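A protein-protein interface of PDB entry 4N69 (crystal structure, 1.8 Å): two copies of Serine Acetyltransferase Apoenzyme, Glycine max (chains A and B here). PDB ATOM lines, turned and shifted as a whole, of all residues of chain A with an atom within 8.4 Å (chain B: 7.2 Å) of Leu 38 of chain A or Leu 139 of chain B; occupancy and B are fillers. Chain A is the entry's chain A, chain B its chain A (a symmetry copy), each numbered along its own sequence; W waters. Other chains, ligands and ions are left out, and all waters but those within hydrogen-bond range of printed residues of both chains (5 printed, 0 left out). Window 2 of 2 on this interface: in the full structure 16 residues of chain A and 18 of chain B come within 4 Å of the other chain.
Of the 20 printed residues of chain A, 4 touch a printed residue of chain B. Hydrophobic or aromatic side chains of chain B within 4 Å of the printed part of chain A: Pro 138 and Leu 139. Among the printed residues, Asp or Glu carboxylates within 4 Å of a Lys or Arg side-chain nitrogen of the other chain: Glu 35 of chain A with Arg 136 of chain B (2.8 Å).
The guanidinium group (NE) of Arg 136 of chain B lies within salt-bridge range of the side-chain carboxylate (OE1) of Glu 35 of chain A (2.8 Å).
Water W4 lies within hydrogen-bond range of OG of Ser 145 of chain B and O of Asn 115 of chain A. Water W5 bridges O of Ala 37 of chain A (2.7 Å) and O of Thr 68 of chain B (3.2 Å). Water W1 lies within hydrogen-bond range of the side-chain carboxylate (OE1) of Glu 35 of chain A, the backbone NH (N) of Leu 139 of chain B and the backbone carbonyl oxygen (O) of Arg 136 of chain B. Water W3 lies within hydrogen-bond range of O of Ser 34 of chain A, OE1 of Glu 35 of chain A and NE of Arg 136 of chain B.
No position is printed for both chains.
The side-chain hydroxyl of Ser 34 of chain A is in hydrogen-bond range of the backbone carbonyl oxygen of Asp 31 of chain A (3.3 Å). OD2 of Asp 31 of chain A is in hydrogen-bond range of NE2 of His 111 of chain A, 2.7 Å away. N of Ala 37 of chain A is in hydrogen-bond range of OE2 of Glu 35 of chain A (3.0 Å). The backbone carbonyl oxygen (O) of Tyr 41 of chain A lies within hydrogen-bond range of the side-chain hydroxyl (OG) of Ser 44 of chain A (3.3 Å). O of Tyr 41 of chain A lies within hydrogen-bond range of OG1 of Thr 45 of chain A, at 2.8 Å.
Of the printed residues of chain B, Asp 31 of chain A touches Pro 138 (3.6 Å). Printed residues of chain B within 4 Å of Glu 35 of chain A: Arg 136 and Leu 139. Of the printed residues of chain B, Tyr 41 of chain A touches Thr 68. Tyr 43 of chain A touches none of the printed residues of chain B. Thr 45 of chain A touches none of the printed residues of chain B. Printed residues of chain A within 4 Å of Thr 68 of chain B: Tyr 41 (3.8 Å). Printed residues of chain A within 4 Å of Arg 136 of chain B: Glu 35 (2.8 Å). Of chain A, only Asp 31 (3.6 Å) and Leu 38 (3.6 Å) come within 4 Å of Pro 138 of chain B. Leu 139 of chain B touches just these residues of chain A: Glu 35 (3.7 Å) and Leu 38 (3.8 Å). The nearest residue of chain B that does not touch Leu 38 of chain A is Ala 142 of chain B (4.2 Å). The nearest residue of chain A that does not touch Leu 139 of chain B is Ala 37 of chain A (4.4 Å). The nearest printed residue of chain A that does not touch Thr 68 of chain B is Leu 38 of chain A (4.3 Å).
Among the printed residues, merely in contact across the chains: Asp 31 of chain A with Pro 138 of chain B (3.6 Å), Leu 38 of chain A with Pro 138 of chain B (3.6 Å), Glu 35 of chain A with Leu 139 of chain B (3.7 Å), Tyr 41 of chain A with Thr 68 of chain B (3.8 Å) and Leu 38 of chain A with Leu 139 of chain B (3.8 Å).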
ATOM      1  N   ALA A  28     -24.237 -21.510 -13.739  1.00  0.00           N
ATOM      2  CA  ALA A  28     -24.935 -20.679 -12.761  1.00  0.00           C
ATOM      3  C   ALA A  28     -24.878 -21.304 -11.367  1.00  0.00           C
ATOM      4  O   ALA A  28     -24.732 -20.605 -10.364  1.00  0.00           O
ATOM      5  CB  ALA A  28     -26.395 -20.452 -13.198  1.00  0.00           C
ATOM      6  N   ASP A  31     -21.517 -20.639  -9.881  1.00  0.00           N
ATOM      7  CA  ASP A  31     -21.441 -19.243  -9.477  1.00  0.00           C
ATOM      8  C   ASP A  31     -22.268 -18.999  -8.216  1.00  0.00           C
ATOM      9  O   ASP A  31     -21.840 -18.272  -7.322  1.00  0.00           O
ATOM     10  CB  ASP A  31     -21.902 -18.313 -10.608  1.00  0.00           C
ATOM     11  CG  ASP A  31     -20.825 -18.089 -11.661  1.00  0.00           C
ATOM     12  OD1 ASP A  31     -19.690 -18.584 -11.486  1.00  0.00           O
ATOM     13  OD2 ASP A  31     -21.113 -17.406 -12.669  1.00  0.00           O
ATOM     14  N   ALA A  32     -23.449 -19.605  -8.131  1.00  0.00           N
ATOM     15  CA  ALA A  32     -24.290 -19.406  -6.949  1.00  0.00           C
ATOM     16  C   ALA A  32     -23.595 -19.979  -5.714  1.00  0.00           C
ATOM     17  O   ALA A  32     -23.609 -19.371  -4.636  1.00  0.00           O
ATOM     18  CB  ALA A  32     -25.656 -20.044  -7.149  1.00  0.00           C
ATOM     19  N   GLU A  33     -22.958 -21.138  -5.876  1.00  0.00           N
ATOM     20  CA  GLU A  33     -22.280 -21.772  -4.751  1.00  0.00           C
ATOM     21  C   GLU A  33     -21.078 -20.959  -4.287  1.00  0.00           C
ATOM     22  O   GLU A  33     -20.749 -20.964  -3.102  1.00  0.00           O
ATOM     23  CB  GLU A  33     -21.852 -23.206  -5.121  1.00  0.00           C
ATOM     24  CG  GLU A  33     -23.055 -24.135  -5.309  1.00  0.00           C
ATOM     25  CD  GLU A  33     -22.706 -25.480  -5.930  1.00  0.00           C
ATOM     26  OE1 GLU A  33     -21.582 -25.638  -6.454  1.00  0.00           O
ATOM     27  OE2 GLU A  33     -23.572 -26.381  -5.907  1.00  0.00           O
ATOM     28  N   SER A  34     -20.429 -20.248  -5.204  1.00  0.00           N
ATOM     29  CA  SER A  34     -19.190 -19.551  -4.851  1.00  0.00           C
ATOM     30  C   SER A  34     -19.437 -18.101  -4.402  1.00  0.00           C
ATOM     31  O   SER A  34     -18.598 -17.520  -3.716  1.00  0.00           O
ATOM     32  CB  SER A  34     -18.198 -19.563  -6.018  1.00  0.00           C
ATOM     33  OG  SER A  34     -18.566 -18.636  -7.022  1.00  0.00           O
ATOM     34  N   GLU A  35     -20.584 -17.531  -4.765  1.00  0.00           N
ATOM     35  CA  GLU A  35     -20.850 -16.122  -4.436  1.00  0.00           C
ATOM     36  C   GLU A  35     -22.233 -15.925  -3.820  1.00  0.00           C
ATOM     37  O   GLU A  35     -23.219 -15.751  -4.527  1.00  0.00           O
ATOM     38  CB  GLU A  35     -20.725 -15.247  -5.681  1.00  0.00           C
ATOM     39  CG  GLU A  35     -20.924 -13.760  -5.406  1.00  0.00           C
ATOM     40  CD  GLU A  35     -20.145 -13.310  -4.176  1.00  0.00           C
ATOM     41  OE1 GLU A  35     -18.897 -13.242  -4.249  1.00  0.00           O
ATOM     42  OE2 GLU A  35     -20.771 -13.050  -3.131  1.00  0.00           O
ATOM     43  N   PRO A  36     -22.304 -15.925  -2.488  1.00  0.00           N
ATOM     44  CA  PRO A  36     -23.610 -15.826  -1.830  1.00  0.00           C
ATOM     45  C   PRO A  36     -24.341 -14.532  -2.136  1.00  0.00           C
ATOM     46  O   PRO A  36     -25.565 -14.542  -2.086  1.00  0.00           O
ATOM     47  CB  PRO A  36     -23.262 -15.943  -0.335  1.00  0.00           C
ATOM     48  CG  PRO A  36     -21.810 -15.718  -0.241  1.00  0.00           C
ATOM     49  CD  PRO A  36     -21.217 -16.182  -1.535  1.00  0.00           C
ATOM     50  N   ALA A  37     -23.639 -13.458  -2.498  1.00  0.00           N
ATOM     51  CA  ALA A  37     -24.342 -12.216  -2.843  1.00  0.00           C
ATOM     52  C   ALA A  37     -25.183 -12.357  -4.114  1.00  0.00           C
ATOM     53  O   ALA A  37     -26.126 -11.595  -4.322  1.00  0.00           O
ATOM     54  CB  ALA A  37     -23.365 -11.059  -3.009  1.00  0.00           C
ATOM     55  N   LEU A  38     -24.828 -13.303  -4.973  1.00  0.00           N
ATOM     56  CA  LEU A  38     -25.523 -13.476  -6.251  1.00  0.00           C
ATOM     57  C   LEU A  38     -26.402 -14.737  -6.295  1.00  0.00           C
ATOM     58  O   LEU A  38     -27.109 -14.963  -7.284  1.00  0.00           O
ATOM     59  CB  LEU A  38     -24.509 -13.537  -7.401  1.00  0.00           C
ATOM     60  CG  LEU A  38     -23.724 -12.246  -7.663  1.00  0.00           C
ATOM     61  CD1 LEU A  38     -22.642 -12.472  -8.707  1.00  0.00           C
ATOM     62  CD2 LEU A  38     -24.672 -11.140  -8.113  1.00  0.00           C
ATOM     63  N   ALA A  39     -26.340 -15.548  -5.245  1.00  0.00           N
ATOM     64  CA  ALA A  39     -26.996 -16.874  -5.258  1.00  0.00           C
ATOM     65  C   ALA A  39     -28.509 -16.802  -5.513  1.00  0.00           C
ATOM     66  O   ALA A  39     -29.044 -17.583  -6.306  1.00  0.00           O
ATOM     67  CB  ALA A  39     -26.730 -17.616  -3.948  1.00  0.00           C
ATOM     68  N   SER A  40     -29.210 -15.895  -4.833  1.00  0.00           N
ATOM     69  CA  SER A  40     -30.664 -15.831  -5.003  1.00  0.00           C
ATOM     70  C   SER A  40     -31.064 -15.345  -6.391  1.00  0.00           C
ATOM     71  O   SER A  40     -32.030 -15.835  -6.980  1.00  0.00           O
ATOM     72  CB  SER A  40     -31.294 -14.936  -3.929  1.00  0.00           C
ATOM     73  OG  SER A  40     -31.111 -15.568  -2.670  1.00  0.00           O
ATOM     74  N   TYR A  41     -30.310 -14.391  -6.903  1.00  0.00           N
ATOM     75  CA  TYR A  41     -30.561 -13.853  -8.234  1.00  0.00           C
ATOM     76  C   TYR A  41     -30.309 -14.929  -9.300  1.00  0.00           C
ATOM     77  O   TYR A  41     -31.064 -15.065 -10.260  1.00  0.00           O
ATOM     78  CB  TYR A  41     -29.689 -12.625  -8.413  1.00  0.00           C
ATOM     79  CG  TYR A  41     -29.258 -12.297  -9.820  1.00  0.00           C
ATOM     80  CD1 TYR A  41     -30.126 -11.650 -10.680  1.00  0.00           C
ATOM     81  CD2 TYR A  41     -27.972 -12.604 -10.269  1.00  0.00           C
ATOM     82  CE1 TYR A  41     -29.743 -11.308 -11.967  1.00  0.00           C
ATOM     83  CE2 TYR A  41     -27.573 -12.268 -11.561  1.00  0.00           C
ATOM     84  CZ  TYR A  41     -28.465 -11.624 -12.402  1.00  0.00           C
ATOM     85  OH  TYR A  41     -28.084 -11.284 -13.686  1.00  0.00           O
ATOM     86  N   LEU A  42     -29.281 -15.745  -9.100  1.00  0.00           N
ATOM     87  CA  LEU A  42     -29.015 -16.819 -10.063  1.00  0.00           C
ATOM     88  C   LEU A  42     -30.103 -17.893  -9.966  1.00  0.00           C
ATOM     89  O   LEU A  42     -30.501 -18.487 -10.971  1.00  0.00           O
ATOM     90  CB  LEU A  42     -27.629 -17.423  -9.826  1.00  0.00           C
ATOM     91  CG  LEU A  42     -26.467 -16.472 -10.137  1.00  0.00           C
ATOM     92  CD1 LEU A  42     -25.142 -17.002  -9.585  1.00  0.00           C
ATOM     93  CD2 LEU A  42     -26.349 -16.266 -11.649  1.00  0.00           C
ATOM     94  N   TYR A  43     -30.595 -18.128  -8.754  1.00  0.00           N
ATOM     95  CA  TYR A  43     -31.689 -19.071  -8.565  1.00  0.00           C
ATOM     96  C   TYR A  43     -32.973 -18.567  -9.241  1.00  0.00           C
ATOM     97  O   TYR A  43     -33.606 -19.301 -10.003  1.00  0.00           O
ATOM     98  CB  TYR A  43     -31.952 -19.332  -7.069  1.00  0.00           C
ATOM     99  CG  TYR A  43     -33.239 -20.084  -6.861  1.00  0.00           C
ATOM    100  CD1 TYR A  43     -33.294 -21.458  -7.073  1.00  0.00           C
ATOM    101  CD2 TYR A  43     -34.413 -19.420  -6.465  1.00  0.00           C
ATOM    102  CE1 TYR A  43     -34.481 -22.170  -6.900  1.00  0.00           C
ATOM    103  CE2 TYR A  43     -35.608 -20.131  -6.289  1.00  0.00           C
ATOM    104  CZ  TYR A  43     -35.622 -21.503  -6.515  1.00  0.00           C
ATOM    105  OH  TYR A  43     -36.778 -22.228  -6.351  1.00  0.00           O
ATOM    106  N   SER A  44     -33.368 -17.330  -8.965  1.00  0.00           N
ATOM    107  CA  SER A  44     -34.633 -16.843  -9.514  1.00  0.00           C
ATOM    108  C   SER A  44     -34.565 -16.716 -11.045  1.00  0.00           C
ATOM    109  O   SER A  44     -35.536 -17.029 -11.731  1.00  0.00           O
ATOM    110  CB  SER A  44     -35.028 -15.504  -8.889  1.00  0.00           C
ATOM    111  OG  SER A  44     -34.120 -14.490  -9.256  1.00  0.00           O
ATOM    112  N   THR A  45     -33.424 -16.277 -11.572  1.00  0.00           N
ATOM    113  CA  THR A  45     -33.292 -16.059 -13.009  1.00  0.00           C
ATOM    114  C   THR A  45     -33.077 -17.353 -13.794  1.00  0.00           C
ATOM    115  O   THR A  45     -33.711 -17.574 -14.833  1.00  0.00           O
ATOM    116  CB  THR A  45     -32.143 -15.079 -13.288  1.00  0.00           C
ATOM    117  OG1 THR A  45     -32.345 -13.901 -12.491  1.00  0.00           O
ATOM    118  CG2 THR A  45     -32.119 -14.679 -14.760  1.00  0.00           C
ATOM    119  N   LEU A  47     -31.722 -20.965 -12.204  1.00  0.00           N
ATOM    120  CA  LEU A  47     -31.806 -22.329 -11.650  1.00  0.00           C
ATOM    121  C   LEU A  47     -33.252 -22.788 -11.366  1.00  0.00           C
ATOM    122  O   LEU A  47     -33.550 -23.986 -11.382  1.00  0.00           O
ATOM    123  CB  LEU A  47     -30.979 -22.418 -10.369  1.00  0.00           C
ATOM    124  CG  LEU A  47     -29.486 -22.127 -10.559  1.00  0.00           C
ATOM    125  CD1 LEU A  47     -28.748 -22.188  -9.215  1.00  0.00           C
ATOM    126  CD2 LEU A  47     -28.849 -23.075 -11.583  1.00  0.00           C
ATOM    127  N   HIS A 111     -22.706 -16.395 -18.606  1.00  0.00           N
ATOM    128  CA  HIS A 111     -22.284 -15.017 -18.391  1.00  0.00           C
ATOM    129  C   HIS A 111     -22.759 -14.174 -19.563  1.00  0.00           C
ATOM    130  O   HIS A 111     -23.101 -13.010 -19.398  1.00  0.00           O
ATOM    131  CB  HIS A 111     -20.775 -14.930 -18.195  1.00  0.00           C
ATOM    132  CG  HIS A 111     -20.307 -15.531 -16.903  1.00  0.00           C
ATOM    133  ND1 HIS A 111     -18.979 -15.810 -16.647  1.00  0.00           N
ATOM    134  CD2 HIS A 111     -20.991 -15.903 -15.794  1.00  0.00           C
ATOM    135  CE1 HIS A 111     -18.868 -16.330 -15.436  1.00  0.00           C
ATOM    136  NE2 HIS A 111     -20.074 -16.394 -14.895  1.00  0.00           N
ATOM    137  N   LEU A 114     -26.507 -13.558 -18.916  1.00  0.00           N
ATOM    138  CA  LEU A 114     -26.784 -12.640 -17.816  1.00  0.00           C
ATOM    139  C   LEU A 114     -26.201 -11.243 -17.978  1.00  0.00           C
ATOM    140  O   LEU A 114     -26.835 -10.262 -17.582  1.00  0.00           O
ATOM    141  CB  LEU A 114     -26.261 -13.223 -16.511  1.00  0.00           C
ATOM    142  CG  LEU A 114     -26.940 -14.502 -16.018  1.00  0.00           C
ATOM    143  CD1 LEU A 114     -26.116 -15.096 -14.893  1.00  0.00           C
ATOM    144  CD2 LEU A 114     -28.351 -14.227 -15.548  1.00  0.00           C
ATOM    145  N   ASN A 115     -24.991 -11.153 -18.529  1.00  0.00           N
ATOM    146  CA  ASN A 115     -24.222  -9.913 -18.440  1.00  0.00           C
ATOM    147  C   ASN A 115     -23.914  -9.215 -19.755  1.00  0.00           C
ATOM    148  O   ASN A 115     -23.515  -8.049 -19.750  1.00  0.00           O
ATOM    149  CB  ASN A 115     -22.887 -10.166 -17.747  1.00  0.00           C
ATOM    150  CG  ASN A 115     -23.045 -10.698 -16.343  1.00  0.00           C
ATOM    151  OD1 ASN A 115     -24.022 -10.395 -15.653  1.00  0.00           O
ATOM    152  ND2 ASN A 115     -22.070 -11.489 -15.904  1.00  0.00           N
ATOM    153  N   THR B  68     -30.970  -6.224  -7.835  1.00  0.00           N
ATOM    154  CA  THR B  68     -30.082  -7.339  -7.511  1.00  0.00           C
ATOM    155  C   THR B  68     -29.202  -7.026  -6.293  1.00  0.00           C
ATOM    156  O   THR B  68     -28.939  -7.900  -5.475  1.00  0.00           O
ATOM    157  CB  THR B  68     -29.184  -7.690  -8.713  1.00  0.00           C
ATOM    158  OG1 THR B  68     -30.002  -7.972  -9.851  1.00  0.00           O
ATOM    159  CG2 THR B  68     -28.285  -8.894  -8.418  1.00  0.00           C
ATOM    160  N   LEU B  69     -28.786  -5.762  -6.170  1.00  0.00           N
ATOM    161  CA  LEU B  69     -27.767  -5.352  -5.204  1.00  0.00           C
ATOM    162  C   LEU B  69     -28.271  -4.224  -4.295  1.00  0.00           C
ATOM    163  O   LEU B  69     -28.396  -3.089  -4.743  1.00  0.00           O
ATOM    164  CB  LEU B  69     -26.491  -4.889  -5.935  1.00  0.00           C
ATOM    165  CG  LEU B  69     -25.851  -5.908  -6.887  1.00  0.00           C
ATOM    166  CD1 LEU B  69     -24.821  -5.234  -7.795  1.00  0.00           C
ATOM    167  CD2 LEU B  69     -25.212  -7.043  -6.106  1.00  0.00           C
ATOM    168  N   LEU B  73     -25.904  -3.273   1.048  1.00  0.00           N
ATOM    169  CA  LEU B  73     -24.902  -4.294   0.762  1.00  0.00           C
ATOM    170  C   LEU B  73     -23.683  -3.686   0.064  1.00  0.00           C
ATOM    171  O   LEU B  73     -22.527  -3.968   0.416  1.00  0.00           O
ATOM    172  CB  LEU B  73     -25.488  -5.394  -0.117  1.00  0.00           C
ATOM    173  CG  LEU B  73     -24.428  -6.379  -0.662  1.00  0.00           C
ATOM    174  CD1 LEU B  73     -23.794  -7.163   0.488  1.00  0.00           C
ATOM    175  CD2 LEU B  73     -25.076  -7.316  -1.639  1.00  0.00           C
ATOM    176  N   LEU B  74     -23.943  -2.885  -0.959  1.00  0.00           N
ATOM    177  CA  LEU B  74     -22.837  -2.249  -1.689  1.00  0.00           C
ATOM    178  C   LEU B  74     -22.077  -1.286  -0.780  1.00  0.00           C
ATOM    179  O   LEU B  74     -20.846  -1.218  -0.828  1.00  0.00           O
ATOM    180  CB  LEU B  74     -23.355  -1.520  -2.925  1.00  0.00           C
ATOM    181  CG  LEU B  74     -23.895  -2.435  -4.031  1.00  0.00           C
ATOM    182  CD1 LEU B  74     -24.408  -1.576  -5.209  1.00  0.00           C
ATOM    183  CD2 LEU B  74     -22.813  -3.414  -4.502  1.00  0.00           C
ATOM    184  N   LEU B  77     -19.760  -3.388   1.144  1.00  0.00           N
ATOM    185  CA  LEU B  77     -18.687  -3.888   0.281  1.00  0.00           C
ATOM    186  C   LEU B  77     -17.613  -2.838   0.053  1.00  0.00           C
ATOM    187  O   LEU B  77     -16.411  -3.111   0.163  1.00  0.00           O
ATOM    188  CB  LEU B  77     -19.256  -4.331  -1.060  1.00  0.00           C
ATOM    189  CG  LEU B  77     -18.254  -4.973  -2.012  1.00  0.00           C
ATOM    190  CD1 LEU B  77     -18.055  -6.448  -1.667  1.00  0.00           C
ATOM    191  CD2 LEU B  77     -18.698  -4.805  -3.461  1.00  0.00           C
ATOM    192  N   ALA B 128     -13.751  -3.400  -7.668  1.00  0.00           N
ATOM    193  CA  ALA B 128     -14.012  -4.540  -8.552  1.00  0.00           C
ATOM    194  C   ALA B 128     -12.718  -5.296  -8.860  1.00  0.00           C
ATOM    195  O   ALA B 128     -12.704  -6.535  -8.932  1.00  0.00           O
ATOM    196  CB  ALA B 128     -14.675  -4.082  -9.858  1.00  0.00           C
ATOM    197  N   LEU B 131     -11.841  -7.378  -5.808  1.00  0.00           N
ATOM    198  CA  LEU B 131     -12.695  -8.572  -5.788  1.00  0.00           C
ATOM    199  C   LEU B 131     -12.194  -9.601  -6.790  1.00  0.00           C
ATOM    200  O   LEU B 131     -12.124 -10.787  -6.483  1.00  0.00           O
ATOM    201  CB  LEU B 131     -14.147  -8.204  -6.100  1.00  0.00           C
ATOM    202  CG  LEU B 131     -14.867  -7.442  -4.996  1.00  0.00           C
ATOM    203  CD1 LEU B 131     -16.188  -6.866  -5.515  1.00  0.00           C
ATOM    204  CD2 LEU B 131     -15.110  -8.368  -3.799  1.00  0.00           C
ATOM    205  N   TRP B 132     -11.857  -9.134  -7.988  1.00  0.00           N
ATOM    206  CA  TRP B 132     -11.315  -9.994  -9.039  1.00  0.00           C
ATOM    207  C   TRP B 132     -10.072 -10.714  -8.549  1.00  0.00           C
ATOM    208  O   TRP B 132      -9.913 -11.919  -8.750  1.00  0.00           O
ATOM    209  CB  TRP B 132     -10.988  -9.165 -10.278  1.00  0.00           C
ATOM    210  CG  TRP B 132     -10.486  -9.947 -11.452  1.00  0.00           C
ATOM    211  CD1 TRP B 132      -9.182 -10.230 -11.761  1.00  0.00           C
ATOM    212  CD2 TRP B 132     -11.279 -10.529 -12.487  1.00  0.00           C
ATOM    213  NE1 TRP B 132      -9.120 -10.959 -12.929  1.00  0.00           N
ATOM    214  CE2 TRP B 132     -10.397 -11.156 -13.393  1.00  0.00           C
ATOM    215  CE3 TRP B 132     -12.658 -10.588 -12.739  1.00  0.00           C
ATOM    216  CZ2 TRP B 132     -10.843 -11.827 -14.527  1.00  0.00           C
ATOM    217  CZ3 TRP B 132     -13.099 -11.259 -13.871  1.00  0.00           C
ATOM    218  CH2 TRP B 132     -12.194 -11.871 -14.746  1.00  0.00           C
ATOM    219  N   ARG B 136     -13.310 -13.390  -6.312  1.00  0.00           N
ATOM    220  CA  ARG B 136     -14.748 -13.154  -6.362  1.00  0.00           C
ATOM    221  C   ARG B 136     -15.093 -12.525  -7.717  1.00  0.00           C
ATOM    222  O   ARG B 136     -15.585 -11.399  -7.794  1.00  0.00           O
ATOM    223  CB  ARG B 136     -15.206 -12.250  -5.203  1.00  0.00           C
ATOM    224  CG  ARG B 136     -15.054 -12.883  -3.805  1.00  0.00           C
ATOM    225  CD  ARG B 136     -15.583 -11.958  -2.695  1.00  0.00           C
ATOM    226  NE  ARG B 136     -17.044 -12.003  -2.536  1.00  0.00           N
ATOM    227  CZ  ARG B 136     -17.713 -11.293  -1.631  1.00  0.00           C
ATOM    228  NH1 ARG B 136     -17.049 -10.478  -0.814  1.00  0.00           N
ATOM    229  NH2 ARG B 136     -19.039 -11.399  -1.530  1.00  0.00           N
ATOM    230  N   ARG B 137     -14.844 -13.276  -8.786  1.00  0.00           N
ATOM    231  CA  ARG B 137     -15.018 -12.747 -10.137  1.00  0.00           C
ATOM    232  C   ARG B 137     -16.476 -12.553 -10.576  1.00  0.00           C
ATOM    233  O   ARG B 137     -16.775 -11.538 -11.199  1.00  0.00           O
ATOM    234  CB  ARG B 137     -14.253 -13.636 -11.130  1.00  0.00           C
ATOM    235  CG  ARG B 137     -12.770 -13.672 -10.785  1.00  0.00           C
ATOM    236  CD  ARG B 137     -11.897 -14.320 -11.848  1.00  0.00           C
ATOM    237  NE  ARG B 137     -10.483 -14.055 -11.567  1.00  0.00           N
ATOM    238  CZ  ARG B 137      -9.472 -14.477 -12.319  1.00  0.00           C
ATOM    239  NH1 ARG B 137      -9.705 -15.199 -13.407  1.00  0.00           N
ATOM    240  NH2 ARG B 137      -8.225 -14.179 -11.978  1.00  0.00           N
ATOM    241  N   PRO B 138     -17.393 -13.491 -10.248  1.00  0.00           N
ATOM    242  CA  PRO B 138     -18.796 -13.180 -10.550  1.00  0.00           C
ATOM    243  C   PRO B 138     -19.263 -11.849  -9.967  1.00  0.00           C
ATOM    244  O   PRO B 138     -19.916 -11.066 -10.663  1.00  0.00           O
ATOM    245  CB  PRO B 138     -19.560 -14.345  -9.901  1.00  0.00           C
ATOM    246  CG  PRO B 138     -18.601 -15.494  -9.994  1.00  0.00           C
ATOM    247  CD  PRO B 138     -17.228 -14.890  -9.802  1.00  0.00           C
ATOM    248  N   LEU B 139     -18.923 -11.589  -8.708  1.00  0.00           N
ATOM    249  CA  LEU B 139     -19.309 -10.338  -8.066  1.00  0.00           C
ATOM    250  C   LEU B 139     -18.564  -9.146  -8.678  1.00  0.00           C
ATOM    251  O   LEU B 139     -19.141  -8.077  -8.869  1.00  0.00           O
ATOM    252  CB  LEU B 139     -19.055 -10.411  -6.556  1.00  0.00           C
ATOM    253  CG  LEU B 139     -19.500  -9.168  -5.787  1.00  0.00           C
ATOM    254  CD1 LEU B 139     -20.990  -8.910  -6.008  1.00  0.00           C
ATOM    255  CD2 LEU B 139     -19.169  -9.287  -4.297  1.00  0.00           C
ATOM    256  N   ALA B 140     -17.287  -9.333  -8.993  1.00  0.00           N
ATOM    257  CA  ALA B 140     -16.505  -8.275  -9.628  1.00  0.00           C
ATOM    258  C   ALA B 140     -17.163  -7.868 -10.930  1.00  0.00           C
ATOM    259  O   ALA B 140     -17.255  -6.689 -11.248  1.00  0.00           O
ATOM    260  CB  ALA B 140     -15.056  -8.738  -9.888  1.00  0.00           C
ATOM    261  N   LEU B 141     -17.628  -8.863 -11.680  1.00  0.00           N
ATOM    262  CA  LEU B 141     -18.252  -8.606 -12.970  1.00  0.00           C
ATOM    263  C   LEU B 141     -19.632  -7.973 -12.801  1.00  0.00           C
ATOM    264  O   LEU B 141     -20.042  -7.131 -13.611  1.00  0.00           O
ATOM    265  CB  LEU B 141     -18.350  -9.898 -13.770  1.00  0.00           C
ATOM    266  CG  LEU B 141     -16.979 -10.418 -14.238  1.00  0.00           C
ATOM    267  CD1 LEU B 141     -17.115 -11.841 -14.754  1.00  0.00           C
ATOM    268  CD2 LEU B 141     -16.402  -9.487 -15.313  1.00  0.00           C
ATOM    269  N   ALA B 142     -20.347  -8.376 -11.754  1.00  0.00           N
ATOM    270  CA  ALA B 142     -21.643  -7.771 -11.459  1.00  0.00           C
ATOM    271  C   ALA B 142     -21.454  -6.292 -11.143  1.00  0.00           C
ATOM    272  O   ALA B 142     -22.217  -5.439 -11.600  1.00  0.00           O
ATOM    273  CB  ALA B 142     -22.335  -8.480 -10.291  1.00  0.00           C
ATOM    274  N   LEU B 143     -20.431  -5.990 -10.356  1.00  0.00           N
ATOM    275  CA  LEU B 143     -20.147  -4.607  -9.991  1.00  0.00           C
ATOM    276  C   LEU B 143     -19.746  -3.822 -11.242  1.00  0.00           C
ATOM    277  O   LEU B 143     -20.207  -2.709 -11.461  1.00  0.00           O
ATOM    278  CB  LEU B 143     -19.040  -4.541  -8.943  1.00  0.00           C
ATOM    279  CG  LEU B 143     -18.540  -3.159  -8.536  1.00  0.00           C
ATOM    280  CD1 LEU B 143     -19.696  -2.242  -8.148  1.00  0.00           C
ATOM    281  CD2 LEU B 143     -17.543  -3.282  -7.387  1.00  0.00           C
ATOM    282  N   HIS B 144     -18.880  -4.423 -12.051  1.00  0.00           N
ATOM    283  CA  HIS B 144     -18.459  -3.844 -13.328  1.00  0.00           C
ATOM    284  C   HIS B 144     -19.642  -3.480 -14.236  1.00  0.00           C
ATOM    285  O   HIS B 144     -19.671  -2.397 -14.818  1.00  0.00           O
ATOM    286  CB  HIS B 144     -17.511  -4.824 -14.025  1.00  0.00           C
ATOM    287  CG  HIS B 144     -17.376  -4.605 -15.496  1.00  0.00           C
ATOM    288  ND1 HIS B 144     -17.934  -5.454 -16.425  1.00  0.00           N
ATOM    289  CD2 HIS B 144     -16.727  -3.649 -16.200  1.00  0.00           C
ATOM    290  CE1 HIS B 144     -17.643  -5.026 -17.639  1.00  0.00           C
ATOM    291  NE2 HIS B 144     -16.911  -3.932 -17.531  1.00  0.00           N
ATOM    292  N   SER B 145     -20.622  -4.374 -14.347  1.00  0.00           N
ATOM    293  CA  SER B 145     -21.800  -4.096 -15.163  1.00  0.00           C
ATOM    294  C   SER B 145     -22.574  -2.869 -14.663  1.00  0.00           C
ATOM    295  O   SER B 145     -23.040  -2.049 -15.473  1.00  0.00           O
ATOM    296  CB  SER B 145     -22.718  -5.318 -15.208  1.00  0.00           C
ATOM    297  OG  SER B 145     -23.881  -5.048 -15.979  1.00  0.00           O
ATOM    298  N   PRO B 157     -12.727  -5.549 -14.851  1.00  0.00           N
ATOM    299  CA  PRO B 157     -12.142  -5.682 -13.511  1.00  0.00           C
ATOM    300  C   PRO B 157     -10.683  -6.106 -13.512  1.00  0.00           C
ATOM    301  O   PRO B 157      -9.970  -5.751 -12.576  1.00  0.00           O
ATOM    302  CB  PRO B 157     -13.015  -6.760 -12.858  1.00  0.00           C
ATOM    303  CG  PRO B 157     -14.332  -6.614 -13.556  1.00  0.00           C
ATOM    304  CD  PRO B 157     -14.001  -6.278 -14.967  1.00  0.00           C
HETATM  305  O   HOH W   1     -17.886 -13.643  -6.879  1.00  0.00           O
HETATM  306  O   HOH W   2     -21.706 -11.903 -12.758  1.00  0.00           O
HETATM  307  O   HOH W   3     -17.524 -15.164  -2.238  1.00  0.00           O
HETATM  308  O   HOH W   4     -24.668  -5.909 -18.383  1.00  0.00           O
HETATM  309  O   HOH W   5     -27.310  -9.419  -3.164  1.00  0.00           O
